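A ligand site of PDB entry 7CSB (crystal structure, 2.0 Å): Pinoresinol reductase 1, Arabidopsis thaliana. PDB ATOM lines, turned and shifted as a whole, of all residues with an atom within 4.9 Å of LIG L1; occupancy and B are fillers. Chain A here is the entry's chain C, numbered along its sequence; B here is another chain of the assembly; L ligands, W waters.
An oxygen (O13) of LG2 L2 is in hydrogen-bond range of the backbone carbonyl oxygen (O) of Gly 91, at 3.2 Å. N of Val 178 sits at hydrogen-bond distance from O2 of LIG L1 (3.1 Å). The side-chain amino group (NZ) of Lys 144 is in hydrogen-bond range of an oxygen (O13) of LG2 L2 (3.0 Å). O5 of LIG L1 lies within hydrogen-bond range of N of Met 125 (2.8 Å).
The side-chain amide nitrogen (ND2) of Asn 173 lies within hydrogen-bond range of the backbone carbonyl oxygen (O) of Tyr 169 (3.0 Å). The side-chain amide nitrogen (ND2) of Asn 173 lies within hydrogen-bond range of the backbone carbonyl oxygen (O) of Gln 176 (3.2 Å). The backbone carbonyl oxygen (O) of Thr 179 lies within hydrogen-bond range of the side-chain amide nitrogen (ND2) of Asn 173. The side-chain amide oxygen of Asn 173 lies close to the backbone carbonyl oxygen of Phe 170, 3.3 Å away.
CG2 of Val 92 touches O4 of LIG L1, at 3.3 Å. CE2 of Phe 94 touches C6 of LIG L1 (3.5 Å). Gly 124 touches LIG L1 (CA to O5, 3.3 Å). Cys 165 touches LIG L1. Tyr 169 touches LIG L1 (O to C1, 3.6 Å). CZ of Phe 170 touches O3 of LIG L1, at 3.4 Å. Asn 173 touches LIG L1. Gln 176 touches LIG L1 (O to C1, 3.8 Å). CE of Met 177 touches O2 of LIG L1 (3.3 Å). O of Thr 179 touches C1 of LIG L1, at 3.5 Å. Gly 273 touches LIG L1. His 276 touches LIG L1 (ND1 to C16, 3.7 Å). Phe 277 touches LIG L1. Ile 280 touches LIG L1. CD2 of Leu 46 of chain B touches O1 of LIG L1 (3.4 Å). Hydrophobic or aromatic side chains that line LIG L1: Val 92, Phe 94, Met 125, Phe 170, Met 177, Val 178, His 276, Phe 277, Ile 280 and Leu 46 of chain B. The nearest printed residue that does not touch LIG L1 is Ala 164 (4.2 Å).
Water W2 bridges the side-chain amino group (NZ) of Lys 144 (2.4 Å) and an oxygen (O5) of LIG L1 (2.5 Å). Water W1 bridges ND1 of His 270 and O2 of LIG L1.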
ATOM      1  N   GLY A  91     -15.685 -12.157 -32.022  1.00  0.00           N
ATOM      2  CA  GLY A  91     -17.123 -12.016 -32.068  1.00  0.00           C
ATOM      3  C   GLY A  91     -17.652 -10.596 -31.937  1.00  0.00           C
ATOM      4  O   GLY A  91     -18.749 -10.383 -31.430  1.00  0.00           O
ATOM      5  N   VAL A  92     -16.897  -9.626 -32.456  1.00  0.00           N
ATOM      6  CA  VAL A  92     -17.245  -8.217 -32.393  1.00  0.00           C
ATOM      7  C   VAL A  92     -17.275  -7.644 -33.808  1.00  0.00           C
ATOM      8  O   VAL A  92     -16.255  -7.686 -34.507  1.00  0.00           O
ATOM      9  CB  VAL A  92     -16.261  -7.411 -31.512  1.00  0.00           C
ATOM     10  CG1 VAL A  92     -16.507  -5.910 -31.698  1.00  0.00           C
ATOM     11  CG2 VAL A  92     -16.379  -7.826 -30.039  1.00  0.00           C
ATOM     12  N   PHE A  94     -17.196  -4.701 -35.129  1.00  0.00           N
ATOM     13  CA  PHE A  94     -16.256  -3.695 -35.602  1.00  0.00           C
ATOM     14  C   PHE A  94     -14.813  -4.190 -35.537  1.00  0.00           C
ATOM     15  O   PHE A  94     -13.916  -3.473 -36.009  1.00  0.00           O
ATOM     16  CB  PHE A  94     -16.399  -2.370 -34.836  1.00  0.00           C
ATOM     17  CG  PHE A  94     -15.890  -2.405 -33.401  1.00  0.00           C
ATOM     18  CD1 PHE A  94     -14.536  -2.267 -33.112  1.00  0.00           C
ATOM     19  CD2 PHE A  94     -16.793  -2.516 -32.342  1.00  0.00           C
ATOM     20  CE1 PHE A  94     -14.096  -2.278 -31.783  1.00  0.00           C
ATOM     21  CE2 PHE A  94     -16.360  -2.517 -31.026  1.00  0.00           C
ATOM     22  CZ  PHE A  94     -15.006  -2.419 -30.747  1.00  0.00           C
ATOM     23  N   GLY A 124     -19.945 -13.245 -22.929  1.00  0.00           N
ATOM     24  CA  GLY A 124     -20.784 -12.056 -23.022  1.00  0.00           C
ATOM     25  C   GLY A 124     -22.200 -12.322 -22.629  1.00  0.00           C
ATOM     26  O   GLY A 124     -22.465 -13.069 -21.674  1.00  0.00           O
ATOM     27  N   MET A 125     -23.128 -11.711 -23.355  1.00  0.00           N
ATOM     28  CA  MET A 125     -24.534 -11.986 -23.135  1.00  0.00           C
ATOM     29  C   MET A 125     -24.819 -13.482 -23.322  1.00  0.00           C
ATOM     30  O   MET A 125     -24.104 -14.185 -24.042  1.00  0.00           O
ATOM     31  CB  MET A 125     -25.392 -11.141 -24.069  1.00  0.00           C
ATOM     32  CG  MET A 125     -25.421  -9.665 -23.628  1.00  0.00           C
ATOM     33  SD  MET A 125     -26.166  -8.588 -24.889  1.00  0.00           S
ATOM     34  CE  MET A 125     -24.787  -8.283 -26.006  1.00  0.00           C
ATOM     35  N   THR A 140     -24.611 -12.363 -33.513  1.00  0.00           N
ATOM     36  CA  THR A 140     -23.747 -12.866 -32.445  1.00  0.00           C
ATOM     37  C   THR A 140     -24.436 -13.994 -31.692  1.00  0.00           C
ATOM     38  O   THR A 140     -23.836 -15.064 -31.461  1.00  0.00           O
ATOM     39  CB  THR A 140     -23.370 -11.713 -31.512  1.00  0.00           C
ATOM     40  OG1 THR A 140     -22.688 -10.703 -32.270  1.00  0.00           O
ATOM     41  CG2 THR A 140     -22.470 -12.184 -30.388  1.00  0.00           C
ATOM     42  N   PHE A 141     -25.696 -13.817 -31.345  1.00  0.00           N
ATOM     43  CA  PHE A 141     -26.372 -14.843 -30.561  1.00  0.00           C
ATOM     44  C   PHE A 141     -26.734 -16.049 -31.407  1.00  0.00           C
ATOM     45  O   PHE A 141     -26.581 -17.187 -30.958  1.00  0.00           O
ATOM     46  CB  PHE A 141     -27.592 -14.241 -29.877  1.00  0.00           C
ATOM     47  CG  PHE A 141     -27.303 -12.885 -29.293  1.00  0.00           C
ATOM     48  CD1 PHE A 141     -26.148 -12.676 -28.572  1.00  0.00           C
ATOM     49  CD2 PHE A 141     -28.144 -11.812 -29.545  1.00  0.00           C
ATOM     50  CE1 PHE A 141     -25.834 -11.424 -28.061  1.00  0.00           C
ATOM     51  CE2 PHE A 141     -27.844 -10.548 -29.023  1.00  0.00           C
ATOM     52  CZ  PHE A 141     -26.690 -10.366 -28.282  1.00  0.00           C
ATOM     53  N   LYS A 144     -23.405 -18.084 -31.940  1.00  0.00           N
ATOM     54  CA  LYS A 144     -22.956 -18.791 -30.741  1.00  0.00           C
ATOM     55  C   LYS A 144     -23.905 -19.932 -30.398  1.00  0.00           C
ATOM     56  O   LYS A 144     -23.467 -20.976 -29.905  1.00  0.00           O
ATOM     57  CB  LYS A 144     -22.806 -17.808 -29.576  1.00  0.00           C
ATOM     58  CG  LYS A 144     -21.597 -16.835 -29.735  1.00  0.00           C
ATOM     59  CD  LYS A 144     -21.511 -15.800 -28.578  1.00  0.00           C
ATOM     60  CE  LYS A 144     -20.271 -14.875 -28.731  1.00  0.00           C
ATOM     61  NZ  LYS A 144     -20.048 -13.946 -27.580  1.00  0.00           N
ATOM     62  N   ALA A 164     -21.033 -10.940 -18.204  1.00  0.00           N
ATOM     63  CA  ALA A 164     -20.483  -9.664 -17.754  1.00  0.00           C
ATOM     64  C   ALA A 164     -20.010  -8.822 -18.944  1.00  0.00           C
ATOM     65  O   ALA A 164     -19.569  -9.378 -19.968  1.00  0.00           O
ATOM     66  CB  ALA A 164     -19.336  -9.884 -16.762  1.00  0.00           C
ATOM     67  N   CYS A 165     -20.185  -7.504 -18.837  1.00  0.00           N
ATOM     68  CA  CYS A 165     -19.584  -6.547 -19.752  1.00  0.00           C
ATOM     69  C   CYS A 165     -18.092  -6.450 -19.457  1.00  0.00           C
ATOM     70  O   CYS A 165     -17.701  -6.241 -18.310  1.00  0.00           O
ATOM     71  CB  CYS A 165     -20.202  -5.154 -19.567  1.00  0.00           C
ATOM     72  SG  CYS A 165     -21.890  -4.894 -20.174  1.00  0.00           S
ATOM     73  N   TYR A 169     -14.757  -1.927 -22.361  1.00  0.00           N
ATOM     74  CA  TYR A 169     -15.735  -1.465 -23.320  1.00  0.00           C
ATOM     75  C   TYR A 169     -16.936  -0.775 -22.689  1.00  0.00           C
ATOM     76  O   TYR A 169     -17.685  -0.110 -23.416  1.00  0.00           O
ATOM     77  CB  TYR A 169     -16.236  -2.627 -24.195  1.00  0.00           C
ATOM     78  CG  TYR A 169     -15.203  -3.067 -25.189  1.00  0.00           C
ATOM     79  CD1 TYR A 169     -14.836  -2.237 -26.250  1.00  0.00           C
ATOM     80  CD2 TYR A 169     -14.528  -4.273 -25.047  1.00  0.00           C
ATOM     81  CE1 TYR A 169     -13.875  -2.616 -27.157  1.00  0.00           C
ATOM     82  CE2 TYR A 169     -13.573  -4.664 -25.959  1.00  0.00           C
ATOM     83  CZ  TYR A 169     -13.249  -3.831 -27.009  1.00  0.00           C
ATOM     84  OH  TYR A 169     -12.274  -4.209 -27.898  1.00  0.00           O
ATOM     85  N   PHE A 170     -17.116  -0.872 -21.381  1.00  0.00           N
ATOM     86  CA  PHE A 170     -18.362  -0.378 -20.808  1.00  0.00           C
ATOM     87  C   PHE A 170     -18.194   0.426 -19.540  1.00  0.00           C
ATOM     88  O   PHE A 170     -19.095   1.205 -19.213  1.00  0.00           O
ATOM     89  CB  PHE A 170     -19.305  -1.543 -20.514  1.00  0.00           C
ATOM     90  CG  PHE A 170     -19.842  -2.233 -21.747  1.00  0.00           C
ATOM     91  CD1 PHE A 170     -21.010  -1.793 -22.367  1.00  0.00           C
ATOM     92  CD2 PHE A 170     -19.205  -3.356 -22.256  1.00  0.00           C
ATOM     93  CE1 PHE A 170     -21.517  -2.455 -23.476  1.00  0.00           C
ATOM     94  CE2 PHE A 170     -19.713  -4.018 -23.365  1.00  0.00           C
ATOM     95  CZ  PHE A 170     -20.874  -3.588 -23.973  1.00  0.00           C
ATOM     96  N   ASN A 173     -15.271   3.978 -20.077  1.00  0.00           N
ATOM     97  CA  ASN A 173     -15.803   5.061 -20.891  1.00  0.00           C
ATOM     98  C   ASN A 173     -17.122   5.593 -20.343  1.00  0.00           C
ATOM     99  O   ASN A 173     -17.860   6.278 -21.067  1.00  0.00           O
ATOM    100  CB  ASN A 173     -15.953   4.601 -22.342  1.00  0.00           C
ATOM    101  CG  ASN A 173     -16.777   3.319 -22.456  1.00  0.00           C
ATOM    102  OD1 ASN A 173     -17.416   2.891 -21.494  1.00  0.00           O
ATOM    103  ND2 ASN A 173     -16.760   2.712 -23.639  1.00  0.00           N
ATOM    104  N   GLN A 176     -20.064   5.336 -22.685  1.00  0.00           N
ATOM    105  CA  GLN A 176     -20.215   6.133 -23.917  1.00  0.00           C
ATOM    106  C   GLN A 176     -19.742   5.338 -25.126  1.00  0.00           C
ATOM    107  O   GLN A 176     -18.656   4.763 -25.102  1.00  0.00           O
ATOM    108  CB  GLN A 176     -19.411   7.443 -23.817  1.00  0.00           C
ATOM    109  CG  GLN A 176     -19.728   8.308 -22.574  1.00  0.00           C
ATOM    110  CD  GLN A 176     -21.200   8.603 -22.442  1.00  0.00           C
ATOM    111  OE1 GLN A 176     -21.721   9.553 -23.025  1.00  0.00           O
ATOM    112  NE2 GLN A 176     -21.900   7.769 -21.687  1.00  0.00           N
ATOM    113  N   MET A 177     -20.537   5.320 -26.208  1.00  0.00           N
ATOM    114  CA  MET A 177     -20.132   4.609 -27.413  1.00  0.00           C
ATOM    115  C   MET A 177     -19.037   5.355 -28.196  1.00  0.00           C
ATOM    116  O   MET A 177     -18.895   6.566 -28.111  1.00  0.00           O
ATOM    117  CB  MET A 177     -21.335   4.374 -28.329  1.00  0.00           C
ATOM    118  CG  MET A 177     -22.435   3.482 -27.696  1.00  0.00           C
ATOM    119  SD  MET A 177     -23.707   2.894 -28.843  1.00  0.00           S
ATOM    120  CE  MET A 177     -22.744   1.839 -29.926  1.00  0.00           C
ATOM    121  N   VAL A 178     -18.249   4.585 -28.959  1.00  0.00           N
ATOM    122  CA  VAL A 178     -17.155   4.994 -29.857  1.00  0.00           C
ATOM    123  C   VAL A 178     -16.017   5.665 -29.085  1.00  0.00           C
ATOM    124  O   VAL A 178     -15.227   6.415 -29.656  1.00  0.00           O
ATOM    125  CB  VAL A 178     -17.651   5.898 -31.016  1.00  0.00           C
ATOM    126  CG1 VAL A 178     -18.880   5.295 -31.707  1.00  0.00           C
ATOM    127  CG2 VAL A 178     -17.921   7.325 -30.547  1.00  0.00           C
ATOM    128  N   THR A 179     -15.925   5.378 -27.795  1.00  0.00           N
ATOM    129  CA  THR A 179     -14.817   5.910 -27.017  1.00  0.00           C
ATOM    130  C   THR A 179     -14.501   4.898 -25.927  1.00  0.00           C
ATOM    131  O   THR A 179     -15.313   4.031 -25.596  1.00  0.00           O
ATOM    132  CB  THR A 179     -15.125   7.306 -26.443  1.00  0.00           C
ATOM    133  OG1 THR A 179     -13.955   7.854 -25.805  1.00  0.00           O
ATOM    134  CG2 THR A 179     -16.258   7.265 -25.429  1.00  0.00           C
ATOM    135  N   LEU A 180     -13.283   4.990 -25.404  1.00  0.00           N
ATOM    136  CA  LEU A 180     -12.786   4.056 -24.398  1.00  0.00           C
ATOM    137  C   LEU A 180     -12.242   4.783 -23.179  1.00  0.00           C
ATOM    138  O   LEU A 180     -11.619   4.154 -22.320  1.00  0.00           O
ATOM    139  CB  LEU A 180     -11.714   3.143 -25.003  1.00  0.00           C
ATOM    140  CG  LEU A 180     -12.202   2.204 -26.121  1.00  0.00           C
ATOM    141  CD1 LEU A 180     -11.049   1.471 -26.769  1.00  0.00           C
ATOM    142  CD2 LEU A 180     -13.268   1.183 -25.577  1.00  0.00           C
ATOM    143  N   HIS A 270     -21.786  -0.473 -36.276  1.00  0.00           N
ATOM    144  CA  HIS A 270     -22.465   0.447 -35.371  1.00  0.00           C
ATOM    145  C   HIS A 270     -23.896   0.004 -35.073  1.00  0.00           C
ATOM    146  O   HIS A 270     -24.347   0.116 -33.924  1.00  0.00           O
ATOM    147  CB  HIS A 270     -22.424   1.859 -35.934  1.00  0.00           C
ATOM    148  CG  HIS A 270     -22.735   2.930 -34.927  1.00  0.00           C
ATOM    149  ND1 HIS A 270     -21.975   3.105 -33.796  1.00  0.00           N
ATOM    150  CD2 HIS A 270     -23.710   3.862 -34.884  1.00  0.00           C
ATOM    151  CE1 HIS A 270     -22.473   4.104 -33.084  1.00  0.00           C
ATOM    152  NE2 HIS A 270     -23.525   4.596 -33.729  1.00  0.00           N
ATOM    153  N   GLY A 273     -23.504  -2.584 -32.399  1.00  0.00           N
ATOM    154  CA  GLY A 273     -23.201  -1.975 -31.121  1.00  0.00           C
ATOM    155  C   GLY A 273     -24.432  -1.384 -30.474  1.00  0.00           C
ATOM    156  O   GLY A 273     -24.732  -1.651 -29.309  1.00  0.00           O
ATOM    157  N   HIS A 276     -26.679  -4.011 -29.105  1.00  0.00           N
ATOM    158  CA  HIS A 276     -26.180  -4.610 -27.876  1.00  0.00           C
ATOM    159  C   HIS A 276     -26.367  -3.661 -26.705  1.00  0.00           C
ATOM    160  O   HIS A 276     -26.857  -4.063 -25.652  1.00  0.00           O
ATOM    161  CB  HIS A 276     -24.723  -5.013 -28.026  1.00  0.00           C
ATOM    162  CG  HIS A 276     -24.537  -6.220 -28.882  1.00  0.00           C
ATOM    163  ND1 HIS A 276     -23.321  -6.853 -29.038  1.00  0.00           N
ATOM    164  CD2 HIS A 276     -25.424  -6.919 -29.627  1.00  0.00           C
ATOM    165  CE1 HIS A 276     -23.460  -7.890 -29.845  1.00  0.00           C
ATOM    166  NE2 HIS A 276     -24.736  -7.949 -30.221  1.00  0.00           N
ATOM    167  N   PHE A 277     -25.972  -2.395 -26.868  1.00  0.00           N
ATOM    168  CA  PHE A 277     -26.169  -1.449 -25.769  1.00  0.00           C
ATOM    169  C   PHE A 277     -27.642  -1.381 -25.363  1.00  0.00           C
ATOM    170  O   PHE A 277     -27.949  -1.247 -24.164  1.00  0.00           O
ATOM    171  CB  PHE A 277     -25.627  -0.077 -26.155  1.00  0.00           C
ATOM    172  CG  PHE A 277     -24.148   0.070 -25.925  1.00  0.00           C
ATOM    173  CD1 PHE A 277     -23.234  -0.627 -26.734  1.00  0.00           C
ATOM    174  CD2 PHE A 277     -23.652   0.904 -24.929  1.00  0.00           C
ATOM    175  CE1 PHE A 277     -21.860  -0.494 -26.547  1.00  0.00           C
ATOM    176  CE2 PHE A 277     -22.272   1.039 -24.701  1.00  0.00           C
ATOM    177  CZ  PHE A 277     -21.371   0.341 -25.528  1.00  0.00           C
ATOM    178  N   ILE A 280     -28.465  -4.262 -23.121  1.00  0.00           N
ATOM    179  CA  ILE A 280     -27.766  -4.208 -21.841  1.00  0.00           C
ATOM    180  C   ILE A 280     -28.325  -3.105 -20.959  1.00  0.00           C
ATOM    181  O   ILE A 280     -28.607  -3.322 -19.769  1.00  0.00           O
ATOM    182  CB  ILE A 280     -26.249  -4.028 -22.041  1.00  0.00           C
ATOM    183  CG1 ILE A 280     -25.631  -5.257 -22.707  1.00  0.00           C
ATOM    184  CG2 ILE A 280     -25.558  -3.709 -20.686  1.00  0.00           C
ATOM    185  CD1 ILE A 280     -24.520  -4.896 -23.724  1.00  0.00           C
ATOM    186  N   LEU A 286     -28.586  -8.354 -18.650  1.00  0.00           N
ATOM    187  CA  LEU A 286     -27.638  -9.023 -17.760  1.00  0.00           C
ATOM    188  C   LEU A 286     -28.131  -9.174 -16.328  1.00  0.00           C
ATOM    189  O   LEU A 286     -27.501  -9.883 -15.534  1.00  0.00           O
ATOM    190  CB  LEU A 286     -26.305  -8.282 -17.733  1.00  0.00           C
ATOM    191  CG  LEU A 286     -25.658  -8.177 -19.097  1.00  0.00           C
ATOM    192  CD1 LEU A 286     -24.410  -7.316 -18.974  1.00  0.00           C
ATOM    193  CD2 LEU A 286     -25.323  -9.599 -19.617  1.00  0.00           C
ATOM    194  N   LEU B  46     -11.863   3.499 -30.799  1.00  0.00           N
ATOM    195  CA  LEU B  46     -11.970   2.155 -30.238  1.00  0.00           C
ATOM    196  C   LEU B  46     -10.706   1.337 -30.406  1.00  0.00           C
ATOM    197  O   LEU B  46     -10.772   0.097 -30.385  1.00  0.00           O
ATOM    198  CB  LEU B  46     -13.161   1.436 -30.851  1.00  0.00           C
ATOM    199  CG  LEU B  46     -14.362   2.174 -30.245  1.00  0.00           C
ATOM    200  CD1 LEU B  46     -14.855   3.216 -31.220  1.00  0.00           C
ATOM    201  CD2 LEU B  46     -15.457   1.278 -29.752  1.00  0.00           C
HETATM  202  C1  LIG L   1     -17.525   1.506 -26.652  1.00  0.00           C
HETATM  203  O1  LIG L   1     -18.229   1.664 -27.887  1.00  0.00           O
HETATM  204  C2  LIG L   1     -18.671   0.515 -28.501  1.00  0.00           C
HETATM  205  C3  LIG L   1     -18.530  -0.793 -28.042  1.00  0.00           C
HETATM  206  C4  LIG L   1     -19.335   0.697 -29.690  1.00  0.00           C
HETATM  207  O2  LIG L   1     -19.475   2.020 -30.112  1.00  0.00           O
HETATM  208  C5  LIG L   1     -19.809  -0.432 -30.377  1.00  0.00           C
HETATM  209  C6  LIG L   1     -19.614  -1.750 -29.908  1.00  0.00           C
HETATM  210  C7  LIG L   1     -19.113  -1.955 -28.624  1.00  0.00           C
HETATM  211  C8  LIG L   1     -18.444  -2.964 -27.870  1.00  0.00           C
HETATM  212  O3  LIG L   1     -20.198  -3.346 -27.274  1.00  0.00           O
HETATM  213  C9  LIG L   1     -20.807  -3.868 -28.645  1.00  0.00           C
HETATM  214  C10 LIG L   1     -19.798  -4.878 -28.113  1.00  0.00           C
HETATM  215  C11 LIG L   1     -18.585  -4.209 -28.085  1.00  0.00           C
HETATM  216  C12 LIG L   1     -17.859  -5.261 -27.420  1.00  0.00           C
HETATM  217  O4  LIG L   1     -17.974  -6.457 -27.549  1.00  0.00           O
HETATM  218  C13 LIG L   1     -19.322  -5.925 -26.949  1.00  0.00           C
HETATM  219  C14 LIG L   1     -20.142  -7.049 -26.669  1.00  0.00           C
HETATM  220  C15 LIG L   1     -20.676  -7.285 -25.394  1.00  0.00           C
HETATM  221  C16 LIG L   1     -20.154  -8.106 -27.569  1.00  0.00           C
HETATM  222  C17 LIG L   1     -20.820  -9.316 -27.338  1.00  0.00           C
HETATM  223  C18 LIG L   1     -21.420  -9.483 -26.065  1.00  0.00           C
HETATM  224  O5  LIG L   1     -22.093 -10.607 -25.696  1.00  0.00           O
HETATM  225  C19 LIG L   1     -21.347  -8.472 -25.114  1.00  0.00           C
HETATM  226  O6  LIG L   1     -21.947  -8.711 -23.896  1.00  0.00           O
HETATM  227  C20 LIG L   1     -21.848  -7.601 -22.992  1.00  0.00           C
HETATM  228  P1  LG2 L   2     -10.493 -10.868 -31.135  1.00  0.00           P
HETATM  229  O1  LG2 L   2     -11.271  -9.941 -32.062  1.00  0.00           O
HETATM  230  O2  LG2 L   2      -9.412 -10.189 -30.297  1.00  0.00           O
HETATM  231  O3  LG2 L   2     -10.231 -12.241 -32.038  1.00  0.00           O
HETATM  232  C1  LG2 L   2      -9.869 -13.272 -31.160  1.00  0.00           C
HETATM  233  C2  LG2 L   2      -9.088 -14.263 -32.029  1.00  0.00           C
HETATM  234  O4  LG2 L   2      -9.856 -14.547 -33.114  1.00  0.00           O
HETATM  235  C3  LG2 L   2      -7.960 -13.659 -32.853  1.00  0.00           C
HETATM  236  O5  LG2 L   2      -6.872 -13.228 -32.083  1.00  0.00           O
HETATM  237  C4  LG2 L   2      -7.681 -14.858 -33.834  1.00  0.00           C
HETATM  238  O6  LG2 L   2      -6.877 -16.059 -33.394  1.00  0.00           O
HETATM  239  C5  LG2 L   2      -8.871 -15.433 -34.005  1.00  0.00           C
HETATM  240  N1  LG2 L   2      -9.490 -15.153 -35.278  1.00  0.00           N
HETATM  241  C6  LG2 L   2     -10.151 -14.108 -35.830  1.00  0.00           C
HETATM  242  N2  LG2 L   2     -10.528 -14.466 -37.055  1.00  0.00           N
HETATM  243  C7  LG2 L   2     -10.116 -15.776 -37.230  1.00  0.00           C
HETATM  244  C8  LG2 L   2     -10.236 -16.596 -38.290  1.00  0.00           C
HETATM  245  N3  LG2 L   2     -10.855 -16.437 -39.592  1.00  0.00           N
HETATM  246  N4  LG2 L   2      -9.758 -17.842 -38.297  1.00  0.00           N
HETATM  247  C9  LG2 L   2      -9.110 -18.303 -37.215  1.00  0.00           C
HETATM  248  N5  LG2 L   2      -8.979 -17.465 -36.131  1.00  0.00           N
HETATM  249  C10 LG2 L   2      -9.471 -16.197 -36.170  1.00  0.00           C
HETATM  250  O7  LG2 L   2     -11.793 -11.254 -30.253  1.00  0.00           O
HETATM  251  P2  LG2 L   2     -12.275 -10.676 -28.782  1.00  0.00           P
HETATM  252  O8  LG2 L   2     -11.399 -11.010 -27.617  1.00  0.00           O
HETATM  253  O9  LG2 L   2     -12.579  -9.198 -28.978  1.00  0.00           O
HETATM  254  O10 LG2 L   2     -13.695 -11.471 -28.619  1.00  0.00           O
HETATM  255  C11 LG2 L   2     -13.587 -12.753 -27.974  1.00  0.00           C
HETATM  256  C12 LG2 L   2     -14.957 -13.170 -27.354  1.00  0.00           C
HETATM  257  O11 LG2 L   2     -15.269 -12.279 -26.402  1.00  0.00           O
HETATM  258  C13 LG2 L   2     -16.041 -13.090 -28.430  1.00  0.00           C
HETATM  259  O12 LG2 L   2     -17.026 -14.055 -28.356  1.00  0.00           O
HETATM  260  C14 LG2 L   2     -16.736 -11.799 -28.042  1.00  0.00           C
HETATM  261  O13 LG2 L   2     -18.095 -11.880 -28.647  1.00  0.00           O
HETATM  262  C15 LG2 L   2     -16.733 -11.751 -26.718  1.00  0.00           C
HETATM  263  N6  LG2 L   2     -16.642 -10.386 -26.201  1.00  0.00           N
HETATM  264  C16 LG2 L   2     -17.527  -9.995 -25.179  1.00  0.00           C
HETATM  265  C17 LG2 L   2     -17.404  -8.663 -24.618  1.00  0.00           C
HETATM  266  C18 LG2 L   2     -18.141  -8.320 -23.374  1.00  0.00           C
HETATM  267  O14 LG2 L   2     -18.711  -9.153 -22.688  1.00  0.00           O
HETATM  268  N7  LG2 L   2     -18.186  -7.000 -23.033  1.00  0.00           N
HETATM  269  C19 LG2 L   2     -16.636  -7.499 -25.253  1.00  0.00           C
HETATM  270  C20 LG2 L   2     -15.785  -8.003 -26.436  1.00  0.00           C
HETATM  271  C21 LG2 L   2     -15.665  -9.496 -26.703  1.00  0.00           C
HETATM  272  P3  LG2 L   2      -5.320 -15.914 -33.164  1.00  0.00           P
HETATM  273  O15 LG2 L   2      -4.758 -15.540 -31.800  1.00  0.00           O
HETATM  274  O16 LG2 L   2      -4.844 -17.296 -33.540  1.00  0.00           O
HETATM  275  O17 LG2 L   2      -4.878 -14.998 -34.271  1.00  0.00           O
HETATM  276  O   HOH W   1     -19.342   1.877 -33.127  1.00  0.00           O
HETATM  277  O   HOH W   2     -22.081 -12.742 -27.069  1.00  0.00           O
